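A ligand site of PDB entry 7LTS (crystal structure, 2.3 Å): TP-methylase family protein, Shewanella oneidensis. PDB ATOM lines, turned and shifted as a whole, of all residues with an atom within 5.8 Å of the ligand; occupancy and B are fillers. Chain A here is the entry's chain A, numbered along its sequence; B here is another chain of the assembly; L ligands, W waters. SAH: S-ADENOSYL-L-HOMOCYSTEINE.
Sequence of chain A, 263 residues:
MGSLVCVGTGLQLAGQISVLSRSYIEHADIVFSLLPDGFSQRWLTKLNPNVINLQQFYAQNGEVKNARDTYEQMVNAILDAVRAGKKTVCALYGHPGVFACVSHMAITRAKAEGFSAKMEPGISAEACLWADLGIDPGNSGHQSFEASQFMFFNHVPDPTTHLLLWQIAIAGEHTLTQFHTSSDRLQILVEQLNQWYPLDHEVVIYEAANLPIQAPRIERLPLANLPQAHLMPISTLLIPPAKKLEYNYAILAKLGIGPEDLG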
ATOM      1  N   LEU A  11     -18.567  -5.140 -22.235  1.00  0.00           N
ATOM      2  CA  LEU A  11     -17.129  -5.033 -21.873  1.00  0.00           C
ATOM      3  C   LEU A  11     -16.810  -5.968 -20.696  1.00  0.00           C
ATOM      4  O   LEU A  11     -15.732  -6.590 -20.718  1.00  0.00           O
ATOM      5  CB  LEU A  11     -16.803  -3.570 -21.550  1.00  0.00           C
ATOM      6  CG  LEU A  11     -16.251  -2.780 -22.734  1.00  0.00           C
ATOM      7  CD1 LEU A  11     -17.182  -2.876 -23.934  1.00  0.00           C
ATOM      8  CD2 LEU A  11     -16.026  -1.327 -22.354  1.00  0.00           C
ATOM      9  N   TYR A  93     -16.904  -7.618 -28.925  1.00  0.00           N
ATOM     10  CA  TYR A  93     -16.958  -7.041 -27.564  1.00  0.00           C
ATOM     11  C   TYR A  93     -17.601  -5.640 -27.673  1.00  0.00           C
ATOM     12  O   TYR A  93     -17.566  -5.028 -28.752  1.00  0.00           O
ATOM     13  CB  TYR A  93     -15.583  -7.047 -26.891  1.00  0.00           C
ATOM     14  CG  TYR A  93     -14.617  -5.988 -27.334  1.00  0.00           C
ATOM     15  CD1 TYR A  93     -13.933  -6.096 -28.530  1.00  0.00           C
ATOM     16  CD2 TYR A  93     -14.364  -4.880 -26.539  1.00  0.00           C
ATOM     17  CE1 TYR A  93     -13.026  -5.129 -28.933  1.00  0.00           C
ATOM     18  CE2 TYR A  93     -13.469  -3.907 -26.921  1.00  0.00           C
ATOM     19  CZ  TYR A  93     -12.793  -4.031 -28.126  1.00  0.00           C
ATOM     20  OH  TYR A  93     -11.902  -3.079 -28.534  1.00  0.00           O
ATOM     21  N   GLY A  94     -18.174  -5.184 -26.560  1.00  0.00           N
ATOM     22  CA  GLY A  94     -18.932  -3.921 -26.497  1.00  0.00           C
ATOM     23  C   GLY A  94     -20.162  -3.980 -27.399  1.00  0.00           C
ATOM     24  O   GLY A  94     -20.954  -4.930 -27.261  1.00  0.00           O
ATOM     25  N   HIS A  95     -20.293  -2.994 -28.284  1.00  0.00           N
ATOM     26  CA  HIS A  95     -21.358  -2.877 -29.310  1.00  0.00           C
ATOM     27  C   HIS A  95     -20.719  -3.135 -30.666  1.00  0.00           C
ATOM     28  O   HIS A  95     -19.759  -2.463 -31.044  1.00  0.00           O
ATOM     29  CB  HIS A  95     -22.029  -1.496 -29.156  1.00  0.00           C
ATOM     30  CG  HIS A  95     -23.153  -1.216 -30.095  1.00  0.00           C
ATOM     31  ND1 HIS A  95     -23.094  -1.509 -31.443  1.00  0.00           N
ATOM     32  CD2 HIS A  95     -24.346  -0.616 -29.887  1.00  0.00           C
ATOM     33  CE1 HIS A  95     -24.213  -1.130 -32.024  1.00  0.00           C
ATOM     34  NE2 HIS A  95     -25.002  -0.580 -31.086  1.00  0.00           N
ATOM     35  N   PRO A  96     -21.207  -4.132 -31.449  1.00  0.00           N
ATOM     36  CA  PRO A  96     -20.546  -4.545 -32.692  1.00  0.00           C
ATOM     37  C   PRO A  96     -20.448  -3.474 -33.792  1.00  0.00           C
ATOM     38  O   PRO A  96     -19.716  -3.693 -34.731  1.00  0.00           O
ATOM     39  CB  PRO A  96     -21.421  -5.695 -33.203  1.00  0.00           C
ATOM     40  CG  PRO A  96     -22.765  -5.450 -32.550  1.00  0.00           C
ATOM     41  CD  PRO A  96     -22.426  -4.908 -31.182  1.00  0.00           C
ATOM     42  N   GLY A  97     -21.186  -2.361 -33.650  1.00  0.00           N
ATOM     43  CA  GLY A  97     -21.222  -1.297 -34.669  1.00  0.00           C
ATOM     44  C   GLY A  97     -20.679   0.020 -34.144  1.00  0.00           C
ATOM     45  O   GLY A  97     -20.738   1.023 -34.891  1.00  0.00           O
ATOM     46  N   VAL A  98     -20.154   0.042 -32.920  1.00  0.00           N
ATOM     47  CA  VAL A  98     -19.593   1.279 -32.282  1.00  0.00           C
ATOM     48  C   VAL A  98     -18.060   1.214 -32.339  1.00  0.00           C
ATOM     49  O   VAL A  98     -17.471   0.344 -31.670  1.00  0.00           O
ATOM     50  CB  VAL A  98     -20.102   1.471 -30.844  1.00  0.00           C
ATOM     51  CG1 VAL A  98     -19.197   2.398 -30.058  1.00  0.00           C
ATOM     52  CG2 VAL A  98     -21.546   1.975 -30.840  1.00  0.00           C
ATOM     53  N   PHE A  99     -17.455   2.112 -33.111  1.00  0.00           N
ATOM     54  CA  PHE A  99     -15.978   2.212 -33.314  1.00  0.00           C
ATOM     55  C   PHE A  99     -15.446   0.835 -33.724  1.00  0.00           C
ATOM     56  O   PHE A  99     -14.429   0.375 -33.156  1.00  0.00           O
ATOM     57  CB  PHE A  99     -15.308   2.765 -32.063  1.00  0.00           C
ATOM     58  CG  PHE A  99     -15.435   4.260 -31.942  1.00  0.00           C
ATOM     59  CD1 PHE A  99     -16.613   4.835 -31.496  1.00  0.00           C
ATOM     60  CD2 PHE A  99     -14.388   5.089 -32.276  1.00  0.00           C
ATOM     61  CE1 PHE A  99     -16.742   6.208 -31.394  1.00  0.00           C
ATOM     62  CE2 PHE A  99     -14.505   6.468 -32.173  1.00  0.00           C
ATOM     63  CZ  PHE A  99     -15.690   7.026 -31.736  1.00  0.00           C
ATOM     64  N   ALA A 100     -16.128   0.212 -34.674  1.00  0.00           N
ATOM     65  CA  ALA A 100     -15.801  -1.091 -35.299  1.00  0.00           C
ATOM     66  C   ALA A 100     -16.549  -1.163 -36.630  1.00  0.00           C
ATOM     67  O   ALA A 100     -17.684  -0.657 -36.683  1.00  0.00           O
ATOM     68  CB  ALA A 100     -16.166  -2.226 -34.379  1.00  0.00           C
ATOM     69  N   ILE A 123     -23.635  -3.161 -25.154  1.00  0.00           N
ATOM     70  CA  ILE A 123     -23.127  -2.123 -24.214  1.00  0.00           C
ATOM     71  C   ILE A 123     -21.681  -1.794 -24.591  1.00  0.00           C
ATOM     72  O   ILE A 123     -20.799  -2.652 -24.420  1.00  0.00           O
ATOM     73  CB  ILE A 123     -23.292  -2.586 -22.759  1.00  0.00           C
ATOM     74  CG1 ILE A 123     -24.771  -2.617 -22.386  1.00  0.00           C
ATOM     75  CG2 ILE A 123     -22.461  -1.713 -21.830  1.00  0.00           C
ATOM     76  CD1 ILE A 123     -25.069  -3.233 -21.033  1.00  0.00           C
ATOM     77  N   SER A 124     -21.484  -0.566 -25.087  1.00  0.00           N
ATOM     78  CA  SER A 124     -20.192  -0.062 -25.613  1.00  0.00           C
ATOM     79  C   SER A 124     -19.379   0.546 -24.473  1.00  0.00           C
ATOM     80  O   SER A 124     -19.908   0.632 -23.345  1.00  0.00           O
ATOM     81  CB  SER A 124     -20.415   0.926 -26.719  1.00  0.00           C
ATOM     82  OG  SER A 124     -20.846   2.179 -26.185  1.00  0.00           O
ATOM     83  N   ALA A 125     -18.140   0.955 -24.754  1.00  0.00           N
ATOM     84  CA  ALA A 125     -17.240   1.560 -23.750  1.00  0.00           C
ATOM     85  C   ALA A 125     -17.816   2.891 -23.262  1.00  0.00           C
ATOM     86  O   ALA A 125     -17.684   3.160 -22.054  1.00  0.00           O
ATOM     87  CB  ALA A 125     -15.843   1.718 -24.312  1.00  0.00           C
ATOM     88  N   GLU A 126     -18.424   3.707 -24.133  1.00  0.00           N
ATOM     89  CA  GLU A 126     -18.973   5.019 -23.702  1.00  0.00           C
ATOM     90  C   GLU A 126     -20.158   4.758 -22.762  1.00  0.00           C
ATOM     91  O   GLU A 126     -20.297   5.518 -21.784  1.00  0.00           O
ATOM     92  CB  GLU A 126     -19.379   5.938 -24.865  1.00  0.00           C
ATOM     93  CG  GLU A 126     -20.238   5.269 -25.922  1.00  0.00           C
ATOM     94  CD  GLU A 126     -21.379   6.130 -26.451  1.00  0.00           C
ATOM     95  OE1 GLU A 126     -21.651   6.070 -27.656  1.00  0.00           O
ATOM     96  OE2 GLU A 126     -21.988   6.857 -25.628  1.00  0.00           O
ATOM     97  N   LEU A 165     -12.274  11.095 -26.784  1.00  0.00           N
ATOM     98  CA  LEU A 165     -11.297  10.705 -27.839  1.00  0.00           C
ATOM     99  C   LEU A 165     -10.978   9.219 -27.637  1.00  0.00           C
ATOM    100  O   LEU A 165     -10.362   8.874 -26.605  1.00  0.00           O
ATOM    101  CB  LEU A 165     -10.053  11.590 -27.759  1.00  0.00           C
ATOM    102  CG  LEU A 165     -10.286  13.073 -28.071  1.00  0.00           C
ATOM    103  CD1 LEU A 165      -8.971  13.845 -28.024  1.00  0.00           C
ATOM    104  CD2 LEU A 165     -10.959  13.255 -29.415  1.00  0.00           C
ATOM    105  N   TRP A 166     -11.408   8.397 -28.590  1.00  0.00           N
ATOM    106  CA  TRP A 166     -11.244   6.926 -28.582  1.00  0.00           C
ATOM    107  C   TRP A 166      -9.855   6.574 -29.121  1.00  0.00           C
ATOM    108  O   TRP A 166      -9.264   7.427 -29.821  1.00  0.00           O
ATOM    109  CB  TRP A 166     -12.352   6.260 -29.412  1.00  0.00           C
ATOM    110  CG  TRP A 166     -13.731   6.495 -28.892  1.00  0.00           C
ATOM    111  CD1 TRP A 166     -14.365   7.702 -28.739  1.00  0.00           C
ATOM    112  CD2 TRP A 166     -14.674   5.504 -28.459  1.00  0.00           C
ATOM    113  NE1 TRP A 166     -15.628   7.519 -28.242  1.00  0.00           N
ATOM    114  CE2 TRP A 166     -15.851   6.182 -28.068  1.00  0.00           C
ATOM    115  CE3 TRP A 166     -14.642   4.104 -28.382  1.00  0.00           C
ATOM    116  CZ2 TRP A 166     -16.971   5.504 -27.591  1.00  0.00           C
ATOM    117  CZ3 TRP A 166     -15.745   3.441 -27.900  1.00  0.00           C
ATOM    118  CH2 TRP A 166     -16.890   4.134 -27.520  1.00  0.00           C
ATOM    119  N   GLN A 167      -9.363   5.370 -28.818  1.00  0.00           N
ATOM    120  CA  GLN A 167      -8.050   4.860 -29.318  1.00  0.00           C
ATOM    121  C   GLN A 167      -6.994   5.943 -29.107  1.00  0.00           C
ATOM    122  O   GLN A 167      -6.244   6.245 -30.052  1.00  0.00           O
ATOM    123  CB  GLN A 167      -8.162   4.478 -30.788  1.00  0.00           C
ATOM    124  CG  GLN A 167      -9.434   3.708 -31.104  1.00  0.00           C
ATOM    125  CD  GLN A 167      -9.318   2.860 -32.353  1.00  0.00           C
ATOM    126  OE1 GLN A 167      -8.728   3.271 -33.343  1.00  0.00           O
ATOM    127  NE2 GLN A 167      -9.888   1.671 -32.297  1.00  0.00           N
ATOM    128  N   ILE A 168      -6.968   6.500 -27.890  1.00  0.00           N
ATOM    129  CA  ILE A 168      -6.064   7.619 -27.505  1.00  0.00           C
ATOM    130  C   ILE A 168      -4.611   7.125 -27.492  1.00  0.00           C
ATOM    131  O   ILE A 168      -3.707   7.950 -27.742  1.00  0.00           O
ATOM    132  CB  ILE A 168      -6.517   8.210 -26.151  1.00  0.00           C
ATOM    133  CG1 ILE A 168      -5.705   9.457 -25.792  1.00  0.00           C
ATOM    134  CG2 ILE A 168      -6.467   7.158 -25.054  1.00  0.00           C
ATOM    135  CD1 ILE A 168      -5.741  10.528 -26.868  1.00  0.00           C
ATOM    136  N   TYR A 206      -9.919   6.760 -18.896  1.00  0.00           N
ATOM    137  CA  TYR A 206     -10.941   5.770 -18.466  1.00  0.00           C
ATOM    138  C   TYR A 206     -10.663   4.424 -19.130  1.00  0.00           C
ATOM    139  O   TYR A 206     -10.479   4.364 -20.357  1.00  0.00           O
ATOM    140  CB  TYR A 206     -12.346   6.248 -18.832  1.00  0.00           C
ATOM    141  CG  TYR A 206     -13.395   5.201 -18.568  1.00  0.00           C
ATOM    142  CD1 TYR A 206     -13.665   4.778 -17.279  1.00  0.00           C
ATOM    143  CD2 TYR A 206     -14.099   4.600 -19.609  1.00  0.00           C
ATOM    144  CE1 TYR A 206     -14.609   3.806 -17.017  1.00  0.00           C
ATOM    145  CE2 TYR A 206     -15.049   3.625 -19.360  1.00  0.00           C
ATOM    146  CZ  TYR A 206     -15.308   3.227 -18.058  1.00  0.00           C
ATOM    147  OH  TYR A 206     -16.250   2.269 -17.800  1.00  0.00           O
ATOM    148  N   GLU A 207     -10.658   3.364 -18.320  1.00  0.00           N
ATOM    149  CA  GLU A 207     -10.580   1.960 -18.797  1.00  0.00           C
ATOM    150  C   GLU A 207     -11.602   1.130 -18.029  1.00  0.00           C
ATOM    151  O   GLU A 207     -11.318   0.762 -16.876  1.00  0.00           O
ATOM    152  CB  GLU A 207      -9.165   1.397 -18.624  1.00  0.00           C
ATOM    153  CG  GLU A 207      -8.095   2.262 -19.271  1.00  0.00           C
ATOM    154  CD  GLU A 207      -6.673   1.779 -19.047  1.00  0.00           C
ATOM    155  OE1 GLU A 207      -6.501   0.760 -18.364  1.00  0.00           O
ATOM    156  OE2 GLU A 207      -5.749   2.440 -19.556  1.00  0.00           O
ATOM    157  N   ALA A 208     -12.753   0.860 -18.649  1.00  0.00           N
ATOM    158  CA  ALA A 208     -13.816  -0.009 -18.091  1.00  0.00           C
ATOM    159  C   ALA A 208     -13.183  -1.364 -17.740  1.00  0.00           C
ATOM    160  O   ALA A 208     -12.306  -1.820 -18.494  1.00  0.00           O
ATOM    161  CB  ALA A 208     -14.942  -0.178 -19.080  1.00  0.00           C
ATOM    162  N   ALA A 209     -13.606  -1.957 -16.620  1.00  0.00           N
ATOM    163  CA  ALA A 209     -13.169  -3.290 -16.166  1.00  0.00           C
ATOM    164  C   ALA A 209     -13.712  -4.351 -17.123  1.00  0.00           C
ATOM    165  O   ALA A 209     -14.877  -4.219 -17.548  1.00  0.00           O
ATOM    166  CB  ALA A 209     -13.634  -3.531 -14.755  1.00  0.00           C
ATOM    167  N   ASN A 210     -12.893  -5.335 -17.460  1.00  0.00           N
ATOM    168  CA  ASN A 210     -13.283  -6.496 -18.316  1.00  0.00           C
ATOM    169  C   ASN A 210     -13.589  -7.686 -17.411  1.00  0.00           C
ATOM    170  O   ASN A 210     -14.238  -8.639 -17.888  1.00  0.00           O
ATOM    171  CB  ASN A 210     -12.192  -6.831 -19.340  1.00  0.00           C
ATOM    172  CG  ASN A 210     -12.069  -5.780 -20.423  1.00  0.00           C
ATOM    173  OD1 ASN A 210     -13.055  -5.472 -21.098  1.00  0.00           O
ATOM    174  ND2 ASN A 210     -10.875  -5.240 -20.593  1.00  0.00           N
ATOM    175  N   MET A 232      -3.143   2.300 -22.608  1.00  0.00           N
ATOM    176  CA  MET A 232      -3.355   0.910 -23.097  1.00  0.00           C
ATOM    177  C   MET A 232      -4.236   0.961 -24.337  1.00  0.00           C
ATOM    178  O   MET A 232      -4.899   1.962 -24.594  1.00  0.00           O
ATOM    179  CB  MET A 232      -4.039   0.064 -22.013  1.00  0.00           C
ATOM    180  CG  MET A 232      -3.236  -0.024 -20.727  1.00  0.00           C
ATOM    181  SD  MET A 232      -1.800  -1.102 -20.885  1.00  0.00           S
ATOM    182  CE  MET A 232      -2.591  -2.699 -20.976  1.00  0.00           C
ATOM    183  N   PRO A 233      -4.267  -0.117 -25.147  1.00  0.00           N
ATOM    184  CA  PRO A 233      -5.194  -0.179 -26.277  1.00  0.00           C
ATOM    185  C   PRO A 233      -6.653   0.037 -25.858  1.00  0.00           C
ATOM    186  O   PRO A 233      -7.444   0.400 -26.709  1.00  0.00           O
ATOM    187  CB  PRO A 233      -4.978  -1.606 -26.806  1.00  0.00           C
ATOM    188  CG  PRO A 233      -3.551  -1.920 -26.424  1.00  0.00           C
ATOM    189  CD  PRO A 233      -3.384  -1.295 -25.064  1.00  0.00           C
ATOM    190  N   ILE A 234      -6.985  -0.173 -24.572  1.00  0.00           N
ATOM    191  CA  ILE A 234      -8.373  -0.083 -24.047  1.00  0.00           C
ATOM    192  C   ILE A 234      -8.624   1.289 -23.410  1.00  0.00           C
ATOM    193  O   ILE A 234      -9.722   1.473 -22.850  1.00  0.00           O
ATOM    194  CB  ILE A 234      -8.671  -1.205 -23.026  1.00  0.00           C
ATOM    195  CG1 ILE A 234      -7.621  -1.251 -21.913  1.00  0.00           C
ATOM    196  CG2 ILE A 234      -8.820  -2.538 -23.740  1.00  0.00           C
ATOM    197  CD1 ILE A 234      -8.138  -1.845 -20.621  1.00  0.00           C
ATOM    198  N   SER A 235      -7.659   2.213 -23.463  1.00  0.00           N
ATOM    199  CA  SER A 235      -7.798   3.569 -22.867  1.00  0.00           C
ATOM    200  C   SER A 235      -8.725   4.429 -23.734  1.00  0.00           C
ATOM    201  O   SER A 235      -8.548   4.450 -24.969  1.00  0.00           O
ATOM    202  CB  SER A 235      -6.459   4.230 -22.702  1.00  0.00           C
ATOM    203  OG  SER A 235      -5.615   3.464 -21.849  1.00  0.00           O
ATOM    204  N   THR A 236      -9.689   5.094 -23.090  1.00  0.00           N
ATOM    205  CA  THR A 236     -10.506   6.175 -23.708  1.00  0.00           C
ATOM    206  C   THR A 236     -10.237   7.463 -22.920  1.00  0.00           C
ATOM    207  O   THR A 236     -10.187   7.392 -21.669  1.00  0.00           O
ATOM    208  CB  THR A 236     -12.007   5.839 -23.751  1.00  0.00           C
ATOM    209  OG1 THR A 236     -12.182   4.685 -24.572  1.00  0.00           O
ATOM    210  CG2 THR A 236     -12.843   6.981 -24.286  1.00  0.00           C
ATOM    211  N   ASP B  58      -7.161  -2.029 -32.645  1.00  0.00           N
ATOM    212  CA  ASP B  58      -7.121  -0.543 -32.648  1.00  0.00           C
ATOM    213  C   ASP B  58      -6.436  -0.054 -33.931  1.00  0.00           C
ATOM    214  O   ASP B  58      -7.060   0.734 -34.668  1.00  0.00           O
ATOM    215  CB  ASP B  58      -6.413   0.015 -31.415  1.00  0.00           C
ATOM    216  CG  ASP B  58      -7.242  -0.107 -30.147  1.00  0.00           C
ATOM    217  OD1 ASP B  58      -8.139  -0.973 -30.123  1.00  0.00           O
ATOM    218  OD2 ASP B  58      -6.973   0.657 -29.202  1.00  0.00           O
ATOM    219  N   TYR B  61      -8.399  -0.684 -37.157  1.00  0.00           N
ATOM    220  CA  TYR B  61      -9.597   0.201 -37.225  1.00  0.00           C
ATOM    221  C   TYR B  61      -9.163   1.645 -37.483  1.00  0.00           C
ATOM    222  O   TYR B  61      -9.768   2.308 -38.344  1.00  0.00           O
ATOM    223  CB  TYR B  61     -10.476   0.087 -35.976  1.00  0.00           C
ATOM    224  CG  TYR B  61     -11.673   0.985 -36.048  1.00  0.00           C
ATOM    225  CD1 TYR B  61     -12.667   0.764 -36.984  1.00  0.00           C
ATOM    226  CD2 TYR B  61     -11.802   2.083 -35.207  1.00  0.00           C
ATOM    227  CE1 TYR B  61     -13.767   1.594 -37.078  1.00  0.00           C
ATOM    228  CE2 TYR B  61     -12.905   2.918 -35.285  1.00  0.00           C
ATOM    229  CZ  TYR B  61     -13.882   2.679 -36.224  1.00  0.00           C
ATOM    230  OH  TYR B  61     -14.971   3.501 -36.314  1.00  0.00           O
HETATM  231  N   SAH L   1     -16.863  -1.746 -30.201  1.00  0.00           N
HETATM  232  CA  SAH L   1     -16.095  -1.396 -28.974  1.00  0.00           C
HETATM  233  CB  SAH L   1     -14.951  -0.424 -29.314  1.00  0.00           C
HETATM  234  CG  SAH L   1     -13.905  -1.018 -30.251  1.00  0.00           C
HETATM  235  SD  SAH L   1     -12.662   0.181 -30.824  1.00  0.00           S
HETATM  236  C   SAH L   1     -17.041  -0.741 -27.962  1.00  0.00           C
HETATM  237  O   SAH L   1     -18.256  -0.793 -28.139  1.00  0.00           O
HETATM  238  OXT SAH L   1     -16.633  -0.174 -26.950  1.00  0.00           O
HETATM  239  C5' SAH L   1     -11.440   0.178 -29.483  1.00  0.00           C
HETATM  240  C4' SAH L   1     -11.538   1.406 -28.613  1.00  0.00           C
HETATM  241  O4' SAH L   1     -12.703   1.308 -27.768  1.00  0.00           O
HETATM  242  C3' SAH L   1     -10.385   1.601 -27.627  1.00  0.00           C
HETATM  243  O3' SAH L   1      -9.255   2.220 -28.231  1.00  0.00           O
HETATM  244  C2' SAH L   1     -11.052   2.524 -26.599  1.00  0.00           C
HETATM  245  O2' SAH L   1     -11.113   3.871 -27.009  1.00  0.00           O
HETATM  246  C1' SAH L   1     -12.426   1.877 -26.511  1.00  0.00           C
HETATM  247  N9  SAH L   1     -12.436   0.842 -25.485  1.00  0.00           N
HETATM  248  C8  SAH L   1     -12.381  -0.515 -25.644  1.00  0.00           C
HETATM  249  N7  SAH L   1     -12.368  -1.168 -24.507  1.00  0.00           N
HETATM  250  C5  SAH L   1     -12.391  -0.173 -23.541  1.00  0.00           C
HETATM  251  C6  SAH L   1     -12.390  -0.223 -22.128  1.00  0.00           C
HETATM  252  N6  SAH L   1     -12.342  -1.346 -21.420  1.00  0.00           N
HETATM  253  N1  SAH L   1     -12.418   0.961 -21.465  1.00  0.00           N
HETATM  254  C2  SAH L   1     -12.456   2.096 -22.181  1.00  0.00           C
HETATM  255  N3  SAH L   1     -12.461   2.259 -23.506  1.00  0.00           N
HETATM  256  C4  SAH L   1     -12.431   1.069 -24.136  1.00  0.00           C
HETATM  257  O   HOH W   1     -12.230  -3.951 -23.946  1.00  0.00           O
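N of Tyr 206 lies within hydrogen-bond range of O of Thr 236, at 2.9 Å.
The backbone carbonyl oxygen of Asp 58 of chain B sits close to the side-chain amide oxygen of Gln 167.
O of Pro 233 sits close to OD2 of Asp 58 of chain B, at 2.6 Å.
N of Gly 97 lies within hydrogen-bond range of ND1 of His 95 (3.0 Å).
OE2 of Glu 207 sits at hydrogen-bond distance from OG of Ser 235 (2.5 Å).
The backbone NH (N) of Met 232 sits at hydrogen-bond distance from the side-chain hydroxyl (OG) of Ser 235.
The backbone carbonyl oxygen of Leu 11 sits close to the side-chain amide oxygen of Asn 210 (2.9 Å).
O of Phe 99 sits close to SD of the ligand.
A nitrogen (N3) of the ligand sits close to the backbone carbonyl oxygen (O) of Ile 234 (2.9 Å).
Merely in contact with the ligand: Leu 11 (3.8 Å), Tyr 93 (3.3 Å), Gly 94 (3.6 Å), Ser 124 (3.1 Å), Trp 166 (3.4 Å), Tyr 206 (3.5 Å) and Glu 207 (3.4 Å).
Of the 29 residues printed, 18 come within 4 Å of the ligand.
A nitrogen (N) of the ligand is in hydrogen-bond range of the backbone carbonyl oxygen (O) of Val 98 (2.6 Å).
N3 of the ligand sits at hydrogen-bond distance from OG1 of Thr 236.
The backbone NH (N) of Ala 208 is in hydrogen-bond range of a nitrogen (N1) of the ligand (2.8 Å).
O of Ala 208 is in hydrogen-bond range of N6 of the ligand, 3.0 Å away.
An oxygen (OXT) of the ligand is in hydrogen-bond range of the backbone NH (N) of Ala 125, at 2.9 Å.
N of Gln 167 lies within hydrogen-bond range of O2' of the ligand, at 2.9 Å.
SD of the ligand lies close to NE2 of Gln 167 (3.5 Å).
An oxygen (O3') of the ligand lies within hydrogen-bond range of the side-chain carboxylate (OD2) of Asp 58 of chain B.
O3' of the ligand is in hydrogen-bond range of O of Pro 233 (3.0 Å).
An oxygen (O) of the ligand lies within hydrogen-bond range of the backbone NH (N) of His 95, 3.0 Å away.
N of the ligand is in hydrogen-bond range of O of His 95.
O2' of the ligand lies within hydrogen-bond range of O of Ser 235 (3.3 Å).
Water W1 bridges N7 of the ligand (2.8 Å) and OD1 of Asn 210 (3.3 Å).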
